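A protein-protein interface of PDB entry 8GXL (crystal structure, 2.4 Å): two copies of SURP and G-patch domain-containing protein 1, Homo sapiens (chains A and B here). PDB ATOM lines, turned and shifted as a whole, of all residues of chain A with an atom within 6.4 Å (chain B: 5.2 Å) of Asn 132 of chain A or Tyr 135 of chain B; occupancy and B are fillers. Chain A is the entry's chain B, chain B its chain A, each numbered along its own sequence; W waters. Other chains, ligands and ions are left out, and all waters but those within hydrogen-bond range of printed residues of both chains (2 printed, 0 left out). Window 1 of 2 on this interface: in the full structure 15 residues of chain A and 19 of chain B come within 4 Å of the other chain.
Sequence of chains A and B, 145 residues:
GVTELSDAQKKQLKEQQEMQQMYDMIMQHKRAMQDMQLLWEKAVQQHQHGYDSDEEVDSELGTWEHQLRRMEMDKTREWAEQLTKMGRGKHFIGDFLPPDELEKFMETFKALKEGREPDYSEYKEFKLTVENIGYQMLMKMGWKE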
ATOM      1  N   PHE A  96     -24.138   8.782 -15.213  1.00  0.00           N
ATOM      2  CA  PHE A  96     -25.235   7.933 -15.645  1.00  0.00           C
ATOM      3  C   PHE A  96     -26.178   7.512 -14.532  1.00  0.00           C
ATOM      4  O   PHE A  96     -27.310   7.121 -14.830  1.00  0.00           O
ATOM      5  CB  PHE A  96     -24.698   6.667 -16.322  1.00  0.00           C
ATOM      6  CG  PHE A  96     -23.993   6.925 -17.615  1.00  0.00           C
ATOM      7  CD1 PHE A  96     -24.718   7.153 -18.775  1.00  0.00           C
ATOM      8  CD2 PHE A  96     -22.605   6.914 -17.682  1.00  0.00           C
ATOM      9  CE1 PHE A  96     -24.072   7.373 -19.992  1.00  0.00           C
ATOM     10  CE2 PHE A  96     -21.950   7.134 -18.888  1.00  0.00           C
ATOM     11  CZ  PHE A  96     -22.689   7.362 -20.049  1.00  0.00           C
ATOM     12  N   LYS A 127     -25.930  -6.173 -13.485  1.00  0.00           N
ATOM     13  CA  LYS A 127     -25.652  -6.609 -14.836  1.00  0.00           C
ATOM     14  C   LYS A 127     -26.458  -5.798 -15.834  1.00  0.00           C
ATOM     15  O   LYS A 127     -25.922  -5.307 -16.826  1.00  0.00           O
ATOM     16  CB  LYS A 127     -25.965  -8.088 -14.952  1.00  0.00           C
ATOM     17  CG  LYS A 127     -26.116  -8.586 -16.357  1.00  0.00           C
ATOM     18  CD  LYS A 127     -26.191 -10.084 -16.310  1.00  0.00           C
ATOM     19  CE  LYS A 127     -26.552 -10.655 -17.639  1.00  0.00           C
ATOM     20  NZ  LYS A 127     -27.103 -12.007 -17.396  1.00  0.00           N
ATOM     21  N   LEU A 128     -27.755  -5.634 -15.576  1.00  0.00           N
ATOM     22  CA  LEU A 128     -28.583  -4.870 -16.498  1.00  0.00           C
ATOM     23  C   LEU A 128     -28.098  -3.436 -16.579  1.00  0.00           C
ATOM     24  O   LEU A 128     -28.119  -2.819 -17.651  1.00  0.00           O
ATOM     25  CB  LEU A 128     -30.040  -4.918 -16.050  1.00  0.00           C
ATOM     26  CG  LEU A 128     -30.804  -6.202 -16.411  1.00  0.00           C
ATOM     27  CD1 LEU A 128     -32.091  -6.299 -15.588  1.00  0.00           C
ATOM     28  CD2 LEU A 128     -31.123  -6.235 -17.908  1.00  0.00           C
ATOM     29  N   THR A 129     -27.622  -2.906 -15.453  1.00  0.00           N
ATOM     30  CA  THR A 129     -27.171  -1.526 -15.397  1.00  0.00           C
ATOM     31  C   THR A 129     -25.893  -1.345 -16.197  1.00  0.00           C
ATOM     32  O   THR A 129     -25.719  -0.326 -16.867  1.00  0.00           O
ATOM     33  CB  THR A 129     -26.956  -1.102 -13.939  1.00  0.00           C
ATOM     34  OG1 THR A 129     -28.163  -1.324 -13.204  1.00  0.00           O
ATOM     35  CG2 THR A 129     -26.539   0.381 -13.854  1.00  0.00           C
ATOM     36  N   VAL A 130     -24.988  -2.322 -16.114  1.00  0.00           N
ATOM     37  CA  VAL A 130     -23.757  -2.282 -16.884  1.00  0.00           C
ATOM     38  C   VAL A 130     -24.068  -2.297 -18.371  1.00  0.00           C
ATOM     39  O   VAL A 130     -23.520  -1.501 -19.149  1.00  0.00           O
ATOM     40  CB  VAL A 130     -22.848  -3.456 -16.488  1.00  0.00           C
ATOM     41  CG1 VAL A 130     -21.800  -3.705 -17.566  1.00  0.00           C
ATOM     42  CG2 VAL A 130     -22.195  -3.161 -15.147  1.00  0.00           C
ATOM     43  N   GLU A 131     -24.958  -3.203 -18.789  1.00  0.00           N
ATOM     44  CA  GLU A 131     -25.316  -3.244 -20.196  1.00  0.00           C
ATOM     45  C   GLU A 131     -26.004  -1.944 -20.606  1.00  0.00           C
ATOM     46  O   GLU A 131     -25.721  -1.397 -21.681  1.00  0.00           O
ATOM     47  CB  GLU A 131     -26.179  -4.476 -20.465  1.00  0.00           C
ATOM     48  CG  GLU A 131     -25.421  -5.787 -20.195  1.00  0.00           C
ATOM     49  CD  GLU A 131     -26.334  -6.970 -19.780  1.00  0.00           C
ATOM     50  OE1 GLU A 131     -27.483  -6.749 -19.310  1.00  0.00           O
ATOM     51  OE2 GLU A 131     -25.884  -8.137 -19.912  1.00  0.00           O
ATOM     52  N   ASN A 132     -26.842  -1.394 -19.715  1.00  0.00           N
ATOM     53  CA  ASN A 132     -27.533  -0.136 -19.974  1.00  0.00           C
ATOM     54  C   ASN A 132     -26.546   1.010 -20.206  1.00  0.00           C
ATOM     55  O   ASN A 132     -26.681   1.772 -21.173  1.00  0.00           O
ATOM     56  CB  ASN A 132     -28.481   0.174 -18.805  1.00  0.00           C
ATOM     57  CG  ASN A 132     -29.382   1.406 -19.056  1.00  0.00           C
ATOM     58  OD1 ASN A 132     -28.966   2.536 -18.820  1.00  0.00           O
ATOM     59  ND2 ASN A 132     -30.618   1.179 -19.510  1.00  0.00           N
ATOM     60  N   ILE A 133     -25.543   1.145 -19.336  1.00  0.00           N
ATOM     61  CA  ILE A 133     -24.552   2.205 -19.510  1.00  0.00           C
ATOM     62  C   ILE A 133     -23.765   2.005 -20.809  1.00  0.00           C
ATOM     63  O   ILE A 133     -23.526   2.960 -21.551  1.00  0.00           O
ATOM     64  CB  ILE A 133     -23.629   2.280 -18.279  1.00  0.00           C
ATOM     65  CG1 ILE A 133     -24.387   2.875 -17.082  1.00  0.00           C
ATOM     66  CG2 ILE A 133     -22.364   3.095 -18.586  1.00  0.00           C
ATOM     67  CD1 ILE A 133     -23.814   2.455 -15.759  1.00  0.00           C
ATOM     68  N   GLY A 134     -23.386   0.758 -21.117  1.00  0.00           N
ATOM     69  CA  GLY A 134     -22.741   0.462 -22.389  1.00  0.00           C
ATOM     70  C   GLY A 134     -23.496   1.020 -23.580  1.00  0.00           C
ATOM     71  O   GLY A 134     -22.911   1.651 -24.465  1.00  0.00           O
ATOM     72  N   TYR A 135     -24.814   0.822 -23.601  1.00  0.00           N
ATOM     73  CA  TYR A 135     -25.625   1.326 -24.706  1.00  0.00           C
ATOM     74  C   TYR A 135     -25.662   2.846 -24.728  1.00  0.00           C
ATOM     75  O   TYR A 135     -25.603   3.458 -25.803  1.00  0.00           O
ATOM     76  CB  TYR A 135     -27.050   0.793 -24.605  1.00  0.00           C
ATOM     77  CG  TYR A 135     -27.159  -0.674 -24.862  1.00  0.00           C
ATOM     78  CD1 TYR A 135     -26.663  -1.228 -26.039  1.00  0.00           C
ATOM     79  CD2 TYR A 135     -27.769  -1.512 -23.938  1.00  0.00           C
ATOM     80  CE1 TYR A 135     -26.770  -2.582 -26.290  1.00  0.00           C
ATOM     81  CE2 TYR A 135     -27.869  -2.883 -24.172  1.00  0.00           C
ATOM     82  CZ  TYR A 135     -27.362  -3.412 -25.338  1.00  0.00           C
ATOM     83  OH  TYR A 135     -27.463  -4.773 -25.574  1.00  0.00           O
ATOM     84  N   GLN A 136     -25.797   3.466 -23.557  1.00  0.00           N
ATOM     85  CA  GLN A 136     -25.844   4.921 -23.486  1.00  0.00           C
ATOM     86  C   GLN A 136     -24.546   5.539 -23.992  1.00  0.00           C
ATOM     87  O   GLN A 136     -24.559   6.611 -24.611  1.00  0.00           O
ATOM     88  CB  GLN A 136     -26.110   5.364 -22.046  1.00  0.00           C
ATOM     89  CG  GLN A 136     -27.568   5.264 -21.643  1.00  0.00           C
ATOM     90  CD  GLN A 136     -27.788   5.829 -20.269  1.00  0.00           C
ATOM     91  OE1 GLN A 136     -27.938   7.033 -20.117  1.00  0.00           O
ATOM     92  NE2 GLN A 136     -27.783   4.968 -19.252  1.00  0.00           N
ATOM     93  N   MET A 137     -23.418   4.876 -23.722  1.00  0.00           N
ATOM     94  CA  MET A 137     -22.123   5.359 -24.178  1.00  0.00           C
ATOM     95  C   MET A 137     -22.015   5.276 -25.689  1.00  0.00           C
ATOM     96  O   MET A 137     -21.590   6.234 -26.344  1.00  0.00           O
ATOM     97  CB  MET A 137     -21.004   4.556 -23.519  1.00  0.00           C
ATOM     98  CG  MET A 137     -20.691   5.013 -22.105  1.00  0.00           C
ATOM     99  SD  MET A 137     -19.715   3.800 -21.203  1.00  0.00           S
ATOM    100  CE  MET A 137     -18.110   4.059 -21.954  1.00  0.00           C
ATOM    101  N   MET A 139     -24.438   5.333 -27.692  1.00  0.00           N
ATOM    102  CA  MET A 139     -25.387   6.308 -28.199  1.00  0.00           C
ATOM    103  C   MET A 139     -24.832   7.724 -28.106  1.00  0.00           C
ATOM    104  O   MET A 139     -25.135   8.553 -28.962  1.00  0.00           O
ATOM    105  CB  MET A 139     -26.713   6.182 -27.438  1.00  0.00           C
ATOM    106  CG  MET A 139     -27.922   6.526 -28.278  1.00  0.00           C
ATOM    107  SD  MET A 139     -29.526   6.450 -27.443  1.00  0.00           S
ATOM    108  CE  MET A 139     -29.251   7.397 -25.936  1.00  0.00           C
ATOM    109  N   ILE B  26     -36.420   7.315 -27.862  1.00  0.00           N
ATOM    110  CA  ILE B  26     -35.556   6.940 -26.748  1.00  0.00           C
ATOM    111  C   ILE B  26     -35.177   8.172 -25.931  1.00  0.00           C
ATOM    112  O   ILE B  26     -35.293   8.180 -24.702  1.00  0.00           O
ATOM    113  CB  ILE B  26     -34.317   6.194 -27.268  1.00  0.00           C
ATOM    114  CG1 ILE B  26     -34.741   4.825 -27.819  1.00  0.00           C
ATOM    115  CG2 ILE B  26     -33.226   6.109 -26.165  1.00  0.00           C
ATOM    116  CD1 ILE B  26     -33.676   4.127 -28.642  1.00  0.00           C
ATOM    117  N   LYS B  30     -36.074   8.901 -22.093  1.00  0.00           N
ATOM    118  CA  LYS B  30     -35.014   9.092 -21.108  1.00  0.00           C
ATOM    119  C   LYS B  30     -35.229  10.378 -20.317  1.00  0.00           C
ATOM    120  O   LYS B  30     -35.126  10.383 -19.084  1.00  0.00           O
ATOM    121  CB  LYS B  30     -33.643   9.095 -21.789  1.00  0.00           C
ATOM    122  CG  LYS B  30     -32.530   9.617 -20.902  1.00  0.00           C
ATOM    123  CD  LYS B  30     -31.244   8.779 -20.994  1.00  0.00           C
ATOM    124  CE  LYS B  30     -30.784   8.576 -22.436  1.00  0.00           C
ATOM    125  NZ  LYS B  30     -29.378   8.066 -22.508  1.00  0.00           N
ATOM    126  N   LEU B 128     -35.081  -1.715 -16.541  1.00  0.00           N
ATOM    127  CA  LEU B 128     -33.791  -1.730 -17.218  1.00  0.00           C
ATOM    128  C   LEU B 128     -33.861  -2.601 -18.458  1.00  0.00           C
ATOM    129  O   LEU B 128     -33.279  -2.266 -19.494  1.00  0.00           O
ATOM    130  CB  LEU B 128     -32.696  -2.201 -16.264  1.00  0.00           C
ATOM    131  CG  LEU B 128     -32.301  -1.235 -15.121  1.00  0.00           C
ATOM    132  CD1 LEU B 128     -31.499  -1.936 -14.027  1.00  0.00           C
ATOM    133  CD2 LEU B 128     -31.513  -0.030 -15.631  1.00  0.00           C
ATOM    134  N   GLU B 131     -35.514  -0.782 -21.259  1.00  0.00           N
ATOM    135  CA  GLU B 131     -34.622   0.215 -21.823  1.00  0.00           C
ATOM    136  C   GLU B 131     -33.557  -0.423 -22.697  1.00  0.00           C
ATOM    137  O   GLU B 131     -33.240   0.100 -23.770  1.00  0.00           O
ATOM    138  CB  GLU B 131     -33.972   1.015 -20.711  1.00  0.00           C
ATOM    139  CG  GLU B 131     -34.949   1.887 -20.010  1.00  0.00           C
ATOM    140  CD  GLU B 131     -34.241   2.988 -19.325  1.00  0.00           C
ATOM    141  OE1 GLU B 131     -33.816   3.925 -20.052  1.00  0.00           O
ATOM    142  OE2 GLU B 131     -34.066   2.882 -18.084  1.00  0.00           O
ATOM    143  N   ASN B 132     -32.981  -1.540 -22.246  1.00  0.00           N
ATOM    144  CA  ASN B 132     -31.936  -2.155 -23.037  1.00  0.00           C
ATOM    145  C   ASN B 132     -32.514  -2.713 -24.323  1.00  0.00           C
ATOM    146  O   ASN B 132     -31.829  -2.729 -25.344  1.00  0.00           O
ATOM    147  CB  ASN B 132     -31.205  -3.222 -22.221  1.00  0.00           C
ATOM    148  CG  ASN B 132     -30.381  -2.620 -21.058  1.00  0.00           C
ATOM    149  OD1 ASN B 132     -30.307  -1.391 -20.889  1.00  0.00           O
ATOM    150  ND2 ASN B 132     -29.781  -3.500 -20.234  1.00  0.00           N
ATOM    151  N   ILE B 133     -33.787  -3.108 -24.314  1.00  0.00           N
ATOM    152  CA  ILE B 133     -34.411  -3.532 -25.559  1.00  0.00           C
ATOM    153  C   ILE B 133     -34.533  -2.350 -26.524  1.00  0.00           C
ATOM    154  O   ILE B 133     -34.215  -2.471 -27.712  1.00  0.00           O
ATOM    155  CB  ILE B 133     -35.769  -4.209 -25.282  1.00  0.00           C
ATOM    156  CG1 ILE B 133     -35.539  -5.552 -24.580  1.00  0.00           C
ATOM    157  CG2 ILE B 133     -36.533  -4.430 -26.603  1.00  0.00           C
ATOM    158  CD1 ILE B 133     -36.794  -6.397 -24.390  1.00  0.00           C
ATOM    159  N   GLY B 134     -34.943  -1.182 -26.024  1.00  0.00           N
ATOM    160  CA  GLY B 134     -34.991   0.001 -26.876  1.00  0.00           C
ATOM    161  C   GLY B 134     -33.632   0.357 -27.459  1.00  0.00           C
ATOM    162  O   GLY B 134     -33.516   0.661 -28.652  1.00  0.00           O
ATOM    163  N   TYR B 135     -32.584   0.303 -26.631  1.00  0.00           N
ATOM    164  CA  TYR B 135     -31.239   0.593 -27.116  1.00  0.00           C
ATOM    165  C   TYR B 135     -30.814  -0.412 -28.173  1.00  0.00           C
ATOM    166  O   TYR B 135     -30.151  -0.052 -29.152  1.00  0.00           O
ATOM    167  CB  TYR B 135     -30.248   0.581 -25.957  1.00  0.00           C
ATOM    168  CG  TYR B 135     -30.369   1.788 -25.055  1.00  0.00           C
ATOM    169  CD1 TYR B 135     -30.314   3.079 -25.578  1.00  0.00           C
ATOM    170  CD2 TYR B 135     -30.546   1.639 -23.670  1.00  0.00           C
ATOM    171  CE1 TYR B 135     -30.432   4.206 -24.749  1.00  0.00           C
ATOM    172  CE2 TYR B 135     -30.662   2.764 -22.828  1.00  0.00           C
ATOM    173  CZ  TYR B 135     -30.609   4.039 -23.379  1.00  0.00           C
ATOM    174  OH  TYR B 135     -30.717   5.149 -22.564  1.00  0.00           O
ATOM    175  N   GLN B 136     -31.193  -1.680 -27.994  1.00  0.00           N
ATOM    176  CA  GLN B 136     -30.778  -2.692 -28.954  1.00  0.00           C
ATOM    177  C   GLN B 136     -31.454  -2.489 -30.309  1.00  0.00           C
ATOM    178  O   GLN B 136     -30.807  -2.659 -31.350  1.00  0.00           O
ATOM    179  CB  GLN B 136     -31.056  -4.088 -28.410  1.00  0.00           C
ATOM    180  CG  GLN B 136     -30.052  -4.545 -27.372  1.00  0.00           C
ATOM    181  CD  GLN B 136     -30.330  -5.950 -26.901  1.00  0.00           C
ATOM    182  OE1 GLN B 136     -29.941  -6.927 -27.548  1.00  0.00           O
ATOM    183  NE2 GLN B 136     -31.042  -6.065 -25.791  1.00  0.00           N
ATOM    184  N   MET B 137     -32.740  -2.100 -30.331  1.00  0.00           N
ATOM    185  CA  MET B 137     -33.368  -1.905 -31.631  1.00  0.00           C
ATOM    186  C   MET B 137     -32.804  -0.675 -32.336  1.00  0.00           C
ATOM    187  O   MET B 137     -32.609  -0.698 -33.552  1.00  0.00           O
ATOM    188  CB  MET B 137     -34.905  -1.870 -31.538  1.00  0.00           C
ATOM    189  CG  MET B 137     -35.550  -1.574 -30.232  1.00  0.00           C
ATOM    190  SD  MET B 137     -37.319  -1.957 -30.191  1.00  0.00           S
ATOM    191  CE  MET B 137     -37.201  -3.724 -30.028  1.00  0.00           C
ATOM    192  N   LEU B 138     -32.499   0.392 -31.595  1.00  0.00           N
ATOM    193  CA  LEU B 138     -31.742   1.484 -32.196  1.00  0.00           C
ATOM    194  C   LEU B 138     -30.424   0.976 -32.759  1.00  0.00           C
ATOM    195  O   LEU B 138     -30.035   1.330 -33.878  1.00  0.00           O
ATOM    196  CB  LEU B 138     -31.472   2.580 -31.169  1.00  0.00           C
ATOM    197  CG  LEU B 138     -30.725   3.743 -31.808  1.00  0.00           C
ATOM    198  CD1 LEU B 138     -31.682   4.484 -32.741  1.00  0.00           C
ATOM    199  CD2 LEU B 138     -30.085   4.673 -30.785  1.00  0.00           C
ATOM    200  N   MET B 139     -29.727   0.142 -31.985  1.00  0.00           N
ATOM    201  CA  MET B 139     -28.425  -0.356 -32.398  1.00  0.00           C
ATOM    202  C   MET B 139     -28.531  -1.174 -33.684  1.00  0.00           C
ATOM    203  O   MET B 139     -27.675  -1.060 -34.568  1.00  0.00           O
ATOM    204  CB  MET B 139     -27.809  -1.188 -31.270  1.00  0.00           C
ATOM    205  CG  MET B 139     -26.304  -1.148 -31.239  1.00  0.00           C
ATOM    206  SD  MET B 139     -25.569  -2.270 -30.034  1.00  0.00           S
ATOM    207  CE  MET B 139     -26.289  -3.824 -30.584  1.00  0.00           C
ATOM    208  N   LYS B 140     -29.582  -1.990 -33.811  1.00  0.00           N
ATOM    209  CA  LYS B 140     -29.770  -2.759 -35.034  1.00  0.00           C
ATOM    210  C   LYS B 140     -29.896  -1.836 -36.238  1.00  0.00           C
ATOM    211  O   LYS B 140     -29.234  -2.045 -37.262  1.00  0.00           O
ATOM    212  CB  LYS B 140     -30.992  -3.673 -34.917  1.00  0.00           C
ATOM    213  CG  LYS B 140     -30.756  -4.922 -34.074  1.00  0.00           C
ATOM    214  CD  LYS B 140     -31.994  -5.828 -33.970  1.00  0.00           C
ATOM    215  CE  LYS B 140     -32.234  -6.649 -35.247  1.00  0.00           C
ATOM    216  NZ  LYS B 140     -33.506  -7.473 -35.234  1.00  0.00           N
HETATM  217  O   HOH W   1     -29.527  -5.963 -21.475  1.00  0.00           O
HETATM  218  O   HOH W   2     -31.110   4.204 -19.897  1.00  0.00           O
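Water W2 lies within hydrogen-bond range of the side-chain carboxylate (OE1) of Glu 131 of chain B (2.7 Å), the side-chain hydroxyl (OH) of Tyr 135 of chain B (2.9 Å), the side-chain amide oxygen (OD1) of Asn 132 of chain A (2.9 Å) and the side-chain amide nitrogen (NE2) of Gln 136 of chain A (3.5 Å). Water W1 bridges ND2 of Asn 132 of chain B (2.8 Å) and OE1 of Glu 131 of chain A (3.1 Å).
The side-chain amino group (NZ) of Lys 30 of chain B is in hydrogen-bond range of the side-chain amide oxygen (OE1) of Gln 136 of chain A (3.0 Å). The backbone carbonyl oxygen of Leu 128 of chain A is in hydrogen-bond range of the side-chain amide nitrogen of Asn 132 of chain B, at 3.1 Å. ND2 of Asn 132 of chain A sits at hydrogen-bond distance from OD1 of Asn 132 of chain B.
Asn 132 of chain A touches just these residues of chain B: Glu 131 (3.6 Å), Asn 132 (2.9 Å) and Tyr 135 (3.7 Å). Tyr 135 of chain B touches four residues of chain A. Of the printed residues of chain A, Gln 136 of chain B touches Tyr 135. Of the printed residues of chain B, Tyr 135 of chain A touches Asn 132, Tyr 135, Gln 136 and Met 139. Printed residues of chain A within 4 Å of Ile 26 of chain B: Met 139 (3.9 Å). The nearest residue of chain B that does not touch Asn 132 of chain A is Leu 128 of chain B (4.2 Å). The nearest printed residue of chain B that does not touch Leu 128 of chain A is Ile 133 of chain B (7.6 Å).
Glu 131 of chain A touches Asn 132 of chain B, and with the chains exchanged Asn 132 of chain A touches Glu 131 of chain B. Asn 132 of chain A touches Tyr 135 of chain B, and with the chains exchanged Tyr 135 of chain A touches Asn 132 of chain B. Tyr 135 of chain A touches Gln 136 of chain B, and with the chains exchanged Gln 136 of chain A touches Tyr 135 of chain B. Tyr 135 of chain A touches Met 139 of chain B, and with the chains exchanged Met 139 of chain A touches Tyr 135 of chain B.
The side-chain amino group of Lys 30 of chain B sits at hydrogen-bond distance from the side-chain hydroxyl of Tyr 135 of chain B (3.2 Å). The side-chain amide oxygen (OD1) of Asn 132 of chain B sits close to the backbone carbonyl oxygen (O) of Leu 128 of chain B (3.4 Å). NE2 of Gln 136 of chain B sits close to O of Asn 132 of chain B, at 3.5 Å. The side-chain amide nitrogen (NE2) of Gln 136 of chain A is in hydrogen-bond range of the side-chain amide oxygen (OD1) of Asn 132 of chain A.
Leu 128 of chain B touches Leu 128 of chain A. OG1 of Thr 129 of chain A touches CD1 of Leu 128 of chain B, at 3.5 Å. ND2 of Asn 132 of chain B touches CB of Glu 131 of chain A, 3.7 Å away. Asn 132 of chain A touches Glu 131 of chain B (ND2 to CB, 3.6 Å). Tyr 135 of chain A touches Asn 132 of chain B. Tyr 135 of chain A touches Tyr 135 of chain B. Tyr 135 of chain A touches Gln 136 of chain B (OH to CG, 3.2 Å). CG of Gln 136 of chain A touches OH of Tyr 135 of chain B, 3.3 Å away. CG2 of Ile 26 of chain B touches SD of Met 139 of chain A (3.9 Å). Met 139 of chain A touches Leu 138 of chain B (CG to CD2, 3.8 Å).
Of the 13 printed residues of chain B, 9 touch a printed residue of chain A. Among the printed residues, 17 pairs touch across the chains.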
